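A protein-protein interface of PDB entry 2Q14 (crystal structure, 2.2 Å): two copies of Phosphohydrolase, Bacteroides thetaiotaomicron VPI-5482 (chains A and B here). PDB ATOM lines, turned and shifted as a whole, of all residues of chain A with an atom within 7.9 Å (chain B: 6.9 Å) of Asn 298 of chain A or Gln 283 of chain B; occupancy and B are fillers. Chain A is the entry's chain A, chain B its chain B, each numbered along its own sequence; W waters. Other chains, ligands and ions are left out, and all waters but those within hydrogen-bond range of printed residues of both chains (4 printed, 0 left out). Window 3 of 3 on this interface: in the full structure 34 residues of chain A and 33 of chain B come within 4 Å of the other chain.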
ATOM      1  N   ALA A 292      10.082 -12.757 -13.189  1.00  0.00           N
ATOM      2  CA  ALA A 292      10.729 -12.931 -14.476  1.00  0.00           C
ATOM      3  C   ALA A 292      10.893 -11.577 -15.173  1.00  0.00           C
ATOM      4  O   ALA A 292      11.977 -11.193 -15.525  1.00  0.00           O
ATOM      5  CB  ALA A 292       9.958 -13.921 -15.346  1.00  0.00           C
ATOM      6  N   LEU A 293       9.819 -10.836 -15.315  1.00  0.00           N
ATOM      7  CA  LEU A 293       9.873  -9.532 -15.963  1.00  0.00           C
ATOM      8  C   LEU A 293      10.883  -8.573 -15.317  1.00  0.00           C
ATOM      9  O   LEU A 293      11.621  -7.882 -16.007  1.00  0.00           O
ATOM     10  CB  LEU A 293       8.494  -8.895 -15.956  1.00  0.00           C
ATOM     11  CG  LEU A 293       7.364  -9.487 -16.795  1.00  0.00           C
ATOM     12  CD1 LEU A 293       6.056  -8.812 -16.402  1.00  0.00           C
ATOM     13  CD2 LEU A 293       7.573  -9.359 -18.358  1.00  0.00           C
ATOM     14  N   LYS A 294      10.907  -8.545 -13.987  1.00  0.00           N
ATOM     15  CA  LYS A 294      11.848  -7.720 -13.249  1.00  0.00           C
ATOM     16  C   LYS A 294      13.308  -8.058 -13.563  1.00  0.00           C
ATOM     17  O   LYS A 294      14.102  -7.173 -13.801  1.00  0.00           O
ATOM     18  CB  LYS A 294      11.598  -7.831 -11.746  1.00  0.00           C
ATOM     19  CG  LYS A 294      10.371  -7.040 -11.233  1.00  0.00           C
ATOM     20  CD  LYS A 294       9.749  -7.670  -9.954  1.00  0.00           C
ATOM     21  CE  LYS A 294      10.755  -7.844  -8.810  1.00  0.00           C
ATOM     22  NZ  LYS A 294      11.130  -6.532  -8.198  1.00  0.00           N
ATOM     23  N   VAL A 295      13.649  -9.333 -13.553  1.00  0.00           N
ATOM     24  CA  VAL A 295      15.020  -9.767 -13.821  1.00  0.00           C
ATOM     25  C   VAL A 295      15.359  -9.650 -15.314  1.00  0.00           C
ATOM     26  O   VAL A 295      16.450  -9.235 -15.688  1.00  0.00           O
ATOM     27  CB  VAL A 295      15.281 -11.206 -13.284  1.00  0.00           C
ATOM     28  CG1 VAL A 295      16.755 -11.576 -13.436  1.00  0.00           C
ATOM     29  CG2 VAL A 295      14.860 -11.285 -11.833  1.00  0.00           C
ATOM     30  N   TRP A 296      14.404  -9.963 -16.166  1.00  0.00           N
ATOM     31  CA  TRP A 296      14.622  -9.882 -17.600  1.00  0.00           C
ATOM     32  C   TRP A 296      14.771  -8.457 -18.062  1.00  0.00           C
ATOM     33  O   TRP A 296      15.260  -8.234 -19.161  1.00  0.00           O
ATOM     34  CB  TRP A 296      13.499 -10.525 -18.387  1.00  0.00           C
ATOM     35  CG  TRP A 296      13.326 -11.962 -18.154  1.00  0.00           C
ATOM     36  CD1 TRP A 296      14.192 -12.826 -17.544  1.00  0.00           C
ATOM     37  CD2 TRP A 296      12.189 -12.716 -18.512  1.00  0.00           C
ATOM     38  NE1 TRP A 296      13.662 -14.079 -17.534  1.00  0.00           N
ATOM     39  CE2 TRP A 296      12.414 -14.028 -18.102  1.00  0.00           C
ATOM     40  CE3 TRP A 296      10.990 -12.403 -19.156  1.00  0.00           C
ATOM     41  CZ2 TRP A 296      11.489 -15.032 -18.313  1.00  0.00           C
ATOM     42  CZ3 TRP A 296      10.072 -13.390 -19.351  1.00  0.00           C
ATOM     43  CH2 TRP A 296      10.324 -14.692 -18.935  1.00  0.00           C
ATOM     44  N   SER A 297      14.349  -7.493 -17.251  1.00  0.00           N
ATOM     45  CA  SER A 297      14.497  -6.109 -17.645  1.00  0.00           C
ATOM     46  C   SER A 297      15.990  -5.699 -17.711  1.00  0.00           C
ATOM     47  O   SER A 297      16.323  -4.697 -18.336  1.00  0.00           O
ATOM     48  CB  SER A 297      13.673  -5.180 -16.757  1.00  0.00           C
ATOM     49  OG  SER A 297      14.270  -5.014 -15.501  1.00  0.00           O
ATOM     50  N   ASN A 298      16.878  -6.481 -17.102  1.00  0.00           N
ATOM     51  CA  ASN A 298      18.314  -6.257 -17.254  1.00  0.00           C
ATOM     52  C   ASN A 298      18.991  -7.300 -18.135  1.00  0.00           C
ATOM     53  O   ASN A 298      20.209  -7.350 -18.169  1.00  0.00           O
ATOM     54  CB  ASN A 298      19.029  -6.215 -15.891  1.00  0.00           C
ATOM     55  CG  ASN A 298      18.432  -5.201 -14.944  1.00  0.00           C
ATOM     56  OD1 ASN A 298      17.918  -5.565 -13.887  1.00  0.00           O
ATOM     57  ND2 ASN A 298      18.472  -3.926 -15.320  1.00  0.00           N
ATOM     58  N   HIS A 299      18.220  -8.116 -18.847  1.00  0.00           N
ATOM     59  CA  HIS A 299      18.800  -9.134 -19.700  1.00  0.00           C
ATOM     60  C   HIS A 299      19.540  -8.473 -20.859  1.00  0.00           C
ATOM     61  O   HIS A 299      19.160  -7.397 -21.285  1.00  0.00           O
ATOM     62  CB  HIS A 299      17.715 -10.046 -20.260  1.00  0.00           C
ATOM     63  CG  HIS A 299      18.231 -11.329 -20.830  1.00  0.00           C
ATOM     64  ND1 HIS A 299      18.628 -11.450 -22.143  1.00  0.00           N
ATOM     65  CD2 HIS A 299      18.382 -12.556 -20.276  1.00  0.00           C
ATOM     66  CE1 HIS A 299      19.009 -12.696 -22.370  1.00  0.00           C
ATOM     67  NE2 HIS A 299      18.867 -13.390 -21.256  1.00  0.00           N
ATOM     68  N   PRO A 300      20.609  -9.112 -21.362  1.00  0.00           N
ATOM     69  CA  PRO A 300      21.312  -8.570 -22.525  1.00  0.00           C
ATOM     70  C   PRO A 300      20.528  -8.521 -23.846  1.00  0.00           C
ATOM     71  O   PRO A 300      20.792  -7.635 -24.662  1.00  0.00           O
ATOM     72  CB  PRO A 300      22.541  -9.480 -22.642  1.00  0.00           C
ATOM     73  CG  PRO A 300      22.680 -10.118 -21.297  1.00  0.00           C
ATOM     74  CD  PRO A 300      21.290 -10.315 -20.843  1.00  0.00           C
ATOM     75  N   ASP A 301      19.580  -9.429 -24.066  1.00  0.00           N
ATOM     76  CA  ASP A 301      18.714  -9.309 -25.226  1.00  0.00           C
ATOM     77  C   ASP A 301      17.976  -7.950 -25.249  1.00  0.00           C
ATOM     78  O   ASP A 301      17.345  -7.553 -24.287  1.00  0.00           O
ATOM     79  CB  ASP A 301      17.718 -10.455 -25.280  1.00  0.00           C
ATOM     80  CG  ASP A 301      16.919 -10.444 -26.554  1.00  0.00           C
ATOM     81  OD1 ASP A 301      17.528 -10.700 -27.597  1.00  0.00           O
ATOM     82  OD2 ASP A 301      15.700 -10.147 -26.534  1.00  0.00           O
ATOM     83  N   LEU A 304      13.743  -8.590 -25.355  1.00  0.00           N
ATOM     84  CA  LEU A 304      13.256  -9.036 -24.073  1.00  0.00           C
ATOM     85  C   LEU A 304      13.355  -7.976 -23.006  1.00  0.00           C
ATOM     86  O   LEU A 304      12.418  -7.786 -22.232  1.00  0.00           O
ATOM     87  CB  LEU A 304      14.033 -10.261 -23.609  1.00  0.00           C
ATOM     88  CG  LEU A 304      13.413 -10.941 -22.383  1.00  0.00           C
ATOM     89  CD1 LEU A 304      12.006 -11.518 -22.738  1.00  0.00           C
ATOM     90  CD2 LEU A 304      14.321 -12.000 -21.806  1.00  0.00           C
ATOM     91  N   SER A 305      14.493  -7.304 -22.943  1.00  0.00           N
ATOM     92  CA  SER A 305      14.718  -6.368 -21.871  1.00  0.00           C
ATOM     93  C   SER A 305      13.930  -5.096 -22.047  1.00  0.00           C
ATOM     94  O   SER A 305      13.515  -4.503 -21.063  1.00  0.00           O
ATOM     95  CB  SER A 305      16.200  -6.044 -21.717  1.00  0.00           C
ATOM     96  OG  SER A 305      16.700  -5.409 -22.866  1.00  0.00           O
ATOM     97  N   THR A 306      13.715  -4.672 -23.288  1.00  0.00           N
ATOM     98  CA  THR A 306      12.968  -3.442 -23.557  1.00  0.00           C
ATOM     99  C   THR A 306      11.488  -3.652 -23.268  1.00  0.00           C
ATOM    100  O   THR A 306      10.822  -2.765 -22.714  1.00  0.00           O
ATOM    101  CB  THR A 306      13.174  -2.982 -25.039  1.00  0.00           C
ATOM    102  OG1 THR A 306      14.555  -2.669 -25.243  1.00  0.00           O
ATOM    103  CG2 THR A 306      12.307  -1.783 -25.404  1.00  0.00           C
ATOM    104  N   SER A 308      10.332  -6.090 -21.205  1.00  0.00           N
ATOM    105  CA  SER A 308      10.281  -6.293 -19.768  1.00  0.00           C
ATOM    106  C   SER A 308      10.327  -5.023 -18.964  1.00  0.00           C
ATOM    107  O   SER A 308       9.586  -4.859 -18.010  1.00  0.00           O
ATOM    108  CB  SER A 308      11.421  -7.199 -19.350  1.00  0.00           C
ATOM    109  OG  SER A 308      11.132  -8.486 -19.823  1.00  0.00           O
ATOM    110  N   LEU A 309      11.198  -4.106 -19.363  1.00  0.00           N
ATOM    111  CA  LEU A 309      11.331  -2.841 -18.658  1.00  0.00           C
ATOM    112  C   LEU A 309      10.099  -1.982 -18.862  1.00  0.00           C
ATOM    113  O   LEU A 309       9.654  -1.286 -17.950  1.00  0.00           O
ATOM    114  CB  LEU A 309      12.606  -2.113 -19.112  1.00  0.00           C
ATOM    115  CG  LEU A 309      13.190  -0.950 -18.316  1.00  0.00           C
ATOM    116  CD1 LEU A 309      13.336  -1.244 -16.849  1.00  0.00           C
ATOM    117  CD2 LEU A 309      14.541  -0.657 -18.936  1.00  0.00           C
ATOM    118  N   ILE A 312       7.454  -3.361 -16.328  1.00  0.00           N
ATOM    119  CA  ILE A 312       7.612  -3.000 -14.925  1.00  0.00           C
ATOM    120  C   ILE A 312       7.627  -1.479 -14.680  1.00  0.00           C
ATOM    121  O   ILE A 312       7.263  -1.015 -13.607  1.00  0.00           O
ATOM    122  CB  ILE A 312       8.818  -3.698 -14.231  1.00  0.00           C
ATOM    123  CG1 ILE A 312      10.143  -3.108 -14.671  1.00  0.00           C
ATOM    124  CG2 ILE A 312       8.777  -5.208 -14.439  1.00  0.00           C
ATOM    125  CD1 ILE A 312      11.324  -3.657 -13.846  1.00  0.00           C
ATOM    126  N   ASN A 313       8.038  -0.696 -15.668  1.00  0.00           N
ATOM    127  CA  ASN A 313       8.081   0.756 -15.488  1.00  0.00           C
ATOM    128  C   ASN A 313       6.872   1.483 -16.045  1.00  0.00           C
ATOM    129  O   ASN A 313       6.807   2.723 -16.016  1.00  0.00           O
ATOM    130  CB  ASN A 313       9.356   1.346 -16.111  1.00  0.00           C
ATOM    131  CG  ASN A 313      10.565   1.116 -15.247  1.00  0.00           C
ATOM    132  OD1 ASN A 313      10.446   0.888 -14.038  1.00  0.00           O
ATOM    133  ND2 ASN A 313      11.725   1.140 -15.853  1.00  0.00           N
ATOM    134  N   ARG B  35       7.305   1.393  -8.764  1.00  0.00           N
ATOM    135  CA  ARG B  35       7.631   0.187  -8.012  1.00  0.00           C
ATOM    136  C   ARG B  35       6.760  -0.025  -6.785  1.00  0.00           C
ATOM    137  O   ARG B  35       6.571  -1.157  -6.360  1.00  0.00           O
ATOM    138  CB  ARG B  35       9.127   0.136  -7.653  1.00  0.00           C
ATOM    139  CG  ARG B  35       9.510   0.839  -6.438  1.00  0.00           C
ATOM    140  CD  ARG B  35      11.033   0.816  -6.207  1.00  0.00           C
ATOM    141  NE  ARG B  35      11.295   0.619  -4.786  1.00  0.00           N
ATOM    142  CZ  ARG B  35      11.070   1.535  -3.840  1.00  0.00           C
ATOM    143  NH1 ARG B  35      10.628   2.776  -4.149  1.00  0.00           N
ATOM    144  NH2 ARG B  35      11.306   1.213  -2.571  1.00  0.00           N
ATOM    145  N   PRO B 102       9.621  -4.143   0.251  1.00  0.00           N
ATOM    146  CA  PRO B 102       8.605  -5.122   0.585  1.00  0.00           C
ATOM    147  C   PRO B 102       8.745  -5.550   2.047  1.00  0.00           C
ATOM    148  O   PRO B 102       9.868  -5.652   2.546  1.00  0.00           O
ATOM    149  CB  PRO B 102       8.889  -6.258  -0.396  1.00  0.00           C
ATOM    150  CG  PRO B 102      10.331  -6.143  -0.659  1.00  0.00           C
ATOM    151  CD  PRO B 102      10.605  -4.678  -0.689  1.00  0.00           C
ATOM    152  N   SER B 255      16.055 -13.959  -6.671  1.00  0.00           N
ATOM    153  CA  SER B 255      16.330 -12.932  -7.669  1.00  0.00           C
ATOM    154  C   SER B 255      17.662 -12.281  -7.302  1.00  0.00           C
ATOM    155  O   SER B 255      18.043 -12.295  -6.140  1.00  0.00           O
ATOM    156  CB  SER B 255      15.215 -11.886  -7.664  1.00  0.00           C
ATOM    157  OG  SER B 255      15.214 -11.131  -6.455  1.00  0.00           O
ATOM    158  N   PRO B 256      18.394 -11.739  -8.290  1.00  0.00           N
ATOM    159  CA  PRO B 256      19.650 -11.076  -7.932  1.00  0.00           C
ATOM    160  C   PRO B 256      19.524 -10.046  -6.829  1.00  0.00           C
ATOM    161  O   PRO B 256      20.336 -10.036  -5.949  1.00  0.00           O
ATOM    162  CB  PRO B 256      20.109 -10.442  -9.237  1.00  0.00           C
ATOM    163  CG  PRO B 256      19.551 -11.416 -10.296  1.00  0.00           C
ATOM    164  CD  PRO B 256      18.181 -11.765  -9.746  1.00  0.00           C
ATOM    165  N   ALA B 257      18.491  -9.214  -6.858  1.00  0.00           N
ATOM    166  CA  ALA B 257      18.306  -8.221  -5.816  1.00  0.00           C
ATOM    167  C   ALA B 257      18.196  -8.845  -4.422  1.00  0.00           C
ATOM    168  O   ALA B 257      18.812  -8.355  -3.483  1.00  0.00           O
ATOM    169  CB  ALA B 257      17.100  -7.334  -6.103  1.00  0.00           C
ATOM    170  N   LEU B 258      17.423  -9.920  -4.288  1.00  0.00           N
ATOM    171  CA  LEU B 258      17.245 -10.560  -2.988  1.00  0.00           C
ATOM    172  C   LEU B 258      18.514 -11.317  -2.564  1.00  0.00           C
ATOM    173  O   LEU B 258      18.890 -11.304  -1.385  1.00  0.00           O
ATOM    174  CB  LEU B 258      16.029 -11.509  -2.999  1.00  0.00           C
ATOM    175  CG  LEU B 258      15.770 -12.371  -1.740  1.00  0.00           C
ATOM    176  CD1 LEU B 258      15.592 -11.496  -0.468  1.00  0.00           C
ATOM    177  CD2 LEU B 258      14.579 -13.308  -1.955  1.00  0.00           C
ATOM    178  N   CYS B 277      24.137  -1.424  -2.529  1.00  0.00           N
ATOM    179  CA  CYS B 277      23.019  -1.676  -1.620  1.00  0.00           C
ATOM    180  C   CYS B 277      21.740  -1.019  -2.111  1.00  0.00           C
ATOM    181  O   CYS B 277      20.744  -1.698  -2.366  1.00  0.00           O
ATOM    182  CB  CYS B 277      23.340  -1.183  -0.212  1.00  0.00           C
ATOM    183  SG  CYS B 277      24.682  -2.099   0.564  1.00  0.00           S
ATOM    184  N   LEU B 278      21.779   0.303  -2.241  1.00  0.00           N
ATOM    185  CA  LEU B 278      20.619   1.054  -2.686  1.00  0.00           C
ATOM    186  C   LEU B 278      20.149   0.549  -4.033  1.00  0.00           C
ATOM    187  O   LEU B 278      18.944   0.371  -4.231  1.00  0.00           O
ATOM    188  CB  LEU B 278      20.905   2.547  -2.773  1.00  0.00           C
ATOM    189  CG  LEU B 278      19.711   3.458  -3.063  1.00  0.00           C
ATOM    190  CD1 LEU B 278      18.648   3.352  -1.976  1.00  0.00           C
ATOM    191  CD2 LEU B 278      20.172   4.914  -3.251  1.00  0.00           C
ATOM    192  N   GLU B 279      21.080   0.303  -4.949  1.00  0.00           N
ATOM    193  CA  GLU B 279      20.705  -0.195  -6.287  1.00  0.00           C
ATOM    194  C   GLU B 279      19.911  -1.491  -6.250  1.00  0.00           C
ATOM    195  O   GLU B 279      18.973  -1.669  -7.004  1.00  0.00           O
ATOM    196  CB  GLU B 279      21.931  -0.462  -7.168  1.00  0.00           C
ATOM    197  CG  GLU B 279      22.688   0.752  -7.563  1.00  0.00           C
ATOM    198  CD  GLU B 279      21.856   1.742  -8.356  1.00  0.00           C
ATOM    199  OE1 GLU B 279      21.078   1.310  -9.238  1.00  0.00           O
ATOM    200  OE2 GLU B 279      22.009   2.958  -8.088  1.00  0.00           O
ATOM    201  N   ASN B 280      20.338  -2.415  -5.406  1.00  0.00           N
ATOM    202  CA  ASN B 280      19.636  -3.677  -5.243  1.00  0.00           C
ATOM    203  C   ASN B 280      18.322  -3.493  -4.460  1.00  0.00           C
ATOM    204  O   ASN B 280      17.323  -4.108  -4.788  1.00  0.00           O
ATOM    205  CB  ASN B 280      20.546  -4.731  -4.582  1.00  0.00           C
ATOM    206  CG  ASN B 280      21.505  -5.360  -5.559  1.00  0.00           C
ATOM    207  OD1 ASN B 280      21.095  -6.163  -6.395  1.00  0.00           O
ATOM    208  ND2 ASN B 280      22.806  -5.016  -5.452  1.00  0.00           N
ATOM    209  N   PHE B 281      18.331  -2.644  -3.446  1.00  0.00           N
ATOM    210  CA  PHE B 281      17.138  -2.406  -2.672  1.00  0.00           C
ATOM    211  C   PHE B 281      15.989  -1.916  -3.557  1.00  0.00           C
ATOM    212  O   PHE B 281      14.866  -2.363  -3.432  1.00  0.00           O
ATOM    213  CB  PHE B 281      17.396  -1.390  -1.566  1.00  0.00           C
ATOM    214  CG  PHE B 281      16.269  -1.279  -0.583  1.00  0.00           C
ATOM    215  CD1 PHE B 281      16.194  -2.141   0.497  1.00  0.00           C
ATOM    216  CD2 PHE B 281      15.275  -0.336  -0.750  1.00  0.00           C
ATOM    217  CE1 PHE B 281      15.151  -2.052   1.407  1.00  0.00           C
ATOM    218  CE2 PHE B 281      14.233  -0.236   0.157  1.00  0.00           C
ATOM    219  CZ  PHE B 281      14.169  -1.103   1.237  1.00  0.00           C
ATOM    220  N   ILE B 282      16.308  -0.976  -4.434  1.00  0.00           N
ATOM    221  CA  ILE B 282      15.389  -0.406  -5.413  1.00  0.00           C
ATOM    222  C   ILE B 282      14.669  -1.453  -6.209  1.00  0.00           C
ATOM    223  O   ILE B 282      13.515  -1.270  -6.561  1.00  0.00           O
ATOM    224  CB  ILE B 282      16.178   0.438  -6.449  1.00  0.00           C
ATOM    225  CG1 ILE B 282      16.404   1.844  -5.968  1.00  0.00           C
ATOM    226  CG2 ILE B 282      15.471   0.520  -7.775  1.00  0.00           C
ATOM    227  CD1 ILE B 282      17.195   2.634  -7.024  1.00  0.00           C
ATOM    228  N   GLN B 283      15.354  -2.553  -6.481  1.00  0.00           N
ATOM    229  CA  GLN B 283      14.808  -3.632  -7.291  1.00  0.00           C
ATOM    230  C   GLN B 283      14.024  -4.684  -6.517  1.00  0.00           C
ATOM    231  O   GLN B 283      13.588  -5.681  -7.097  1.00  0.00           O
ATOM    232  CB  GLN B 283      15.944  -4.329  -8.039  1.00  0.00           C
ATOM    233  CG  GLN B 283      16.872  -3.380  -8.744  1.00  0.00           C
ATOM    234  CD  GLN B 283      17.090  -3.756 -10.147  1.00  0.00           C
ATOM    235  OE1 GLN B 283      18.131  -4.307 -10.501  1.00  0.00           O
ATOM    236  NE2 GLN B 283      16.090  -3.501 -10.975  1.00  0.00           N
ATOM    237  N   LEU B 284      13.862  -4.481  -5.213  1.00  0.00           N
ATOM    238  CA  LEU B 284      13.063  -5.375  -4.399  1.00  0.00           C
ATOM    239  C   LEU B 284      11.607  -4.945  -4.321  1.00  0.00           C
ATOM    240  O   LEU B 284      11.300  -3.776  -4.089  1.00  0.00           O
ATOM    241  CB  LEU B 284      13.597  -5.458  -2.982  1.00  0.00           C
ATOM    242  CG  LEU B 284      14.903  -6.143  -2.646  1.00  0.00           C
ATOM    243  CD1 LEU B 284      15.172  -5.887  -1.192  1.00  0.00           C
ATOM    244  CD2 LEU B 284      14.902  -7.640  -2.960  1.00  0.00           C
ATOM    245  N   ASP B 285      10.710  -5.907  -4.479  1.00  0.00           N
ATOM    246  CA  ASP B 285       9.313  -5.684  -4.166  1.00  0.00           C
ATOM    247  C   ASP B 285       8.710  -7.003  -3.686  1.00  0.00           C
ATOM    248  O   ASP B 285       9.427  -7.944  -3.453  1.00  0.00           O
ATOM    249  CB  ASP B 285       8.578  -5.025  -5.342  1.00  0.00           C
ATOM    250  CG  ASP B 285       8.610  -5.851  -6.585  1.00  0.00           C
ATOM    251  OD1 ASP B 285       8.326  -7.058  -6.497  1.00  0.00           O
ATOM    252  OD2 ASP B 285       8.926  -5.294  -7.648  1.00  0.00           O
ATOM    253  N   ASP B 288       9.634 -10.461  -5.201  1.00  0.00           N
ATOM    254  CA  ASP B 288      10.891 -11.116  -4.860  1.00  0.00           C
ATOM    255  C   ASP B 288      10.757 -11.978  -3.613  1.00  0.00           C
ATOM    256  O   ASP B 288      11.373 -13.038  -3.508  1.00  0.00           O
ATOM    257  CB  ASP B 288      12.043 -10.117  -4.634  1.00  0.00           C
ATOM    258  CG  ASP B 288      12.310  -9.246  -5.818  1.00  0.00           C
ATOM    259  OD1 ASP B 288      13.028  -9.675  -6.728  1.00  0.00           O
ATOM    260  OD2 ASP B 288      11.819  -8.105  -5.832  1.00  0.00           O
HETATM  261  O   HOH W   1      15.798  -2.611 -13.914  1.00  0.00           O
HETATM  262  O   HOH W   2      14.134  -8.181  -8.335  1.00  0.00           O
HETATM  263  O   HOH W   3      12.511  -4.867  -9.982  1.00  0.00           O
HETATM  264  O   HOH W   4       9.204   0.573 -11.409  1.00  0.00           O
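Among the printed residues, merely in contact across the chains: Asn 298 of chain A with Gln 283 of chain B (3.6 Å) and Val 295 of chain A with Pro 256 of chain B (3.95 Å).
Water W2 lies within hydrogen-bond range of OD1 of Asp 288 of chain B (2.5 Å), O of Gln 283 of chain B (2.8 Å) and NZ of Lys 294 of chain A (3.4 Å).
Water W3 bridges the side-chain amino group of Lys 294 of chain A (2.8 Å) and the backbone carbonyl oxygen of Gln 283 of chain B (3.2 Å).
Water W4 lies within hydrogen-bond range of the side-chain amide oxygen of Asn 313 of chain A (2.9 Å), the backbone carbonyl oxygen of Ile 312 of chain A (3.3 Å) and the backbone NH of Arg 35 of chain B (3.4 Å).
Water W1 lies within hydrogen-bond range of the side-chain amide nitrogen (NE2) of Gln 283 of chain B, the side-chain hydroxyl (OG) of Ser 297 of chain A and the side-chain amide nitrogen (ND2) of Asn 298 of chain A.
Printed residues of chain B within 4 Å of Lys 294 of chain A: Gln 283, Asp 285 and Asp 288.
Of the printed residues of chain B, Val 295 of chain A touches Pro 256 (3.95 Å).
Asn 298 of chain A touches just one residue of chain B: Gln 283 (3.6 Å).
Printed residues of chain A within 4 Å of Pro 256 of chain B: Val 295 (3.95 Å).
Gln 283 of chain B touches just these residues of chain A: Lys 294 and Asn 298.
Of the printed residues of chain A, Asp 285 of chain B touches Lys 294 (2.6 Å).
Printed residues of chain A within 4 Å of Asp 288 of chain B: Lys 294 (2.9 Å).
The nearest printed residue of chain A that does not touch Asp 288 of chain B is Val 295 of chain A (5.7 Å).
No position is printed for both chains.
Hydrophobic or aromatic side chains of chain A within 4 Å of the printed part of chain B: Val 295.
Along chain A the printed residues that touch a printed residue of chain B span positions 294 to 298.
Among the printed residues, 5 pairs touch across the chains.
The backbone carbonyl oxygen of Gln 283 of chain B sits at hydrogen-bond distance from the side-chain amino group of Lys 294 of chain A (2.8 Å).
OD2 of Asp 285 of chain B is in salt-bridge range of NZ of Lys 294 of chain A, at 2.6 Å.
The side-chain carboxylate (OD2) of Asp 288 of chain B is in salt-bridge range of the side-chain amino group (NZ) of Lys 294 of chain A (2.9 Å).
OG of Ser 297 of chain A lies within hydrogen-bond range of O of Lys 294 of chain A, at 2.8 Å.
OD1 of Asp 288 of chain B lies within hydrogen-bond range of OG of Ser 255 of chain B (2.6 Å).
OD2 of Asp 288 of chain B sits at hydrogen-bond distance from N of Asp 285 of chain B.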
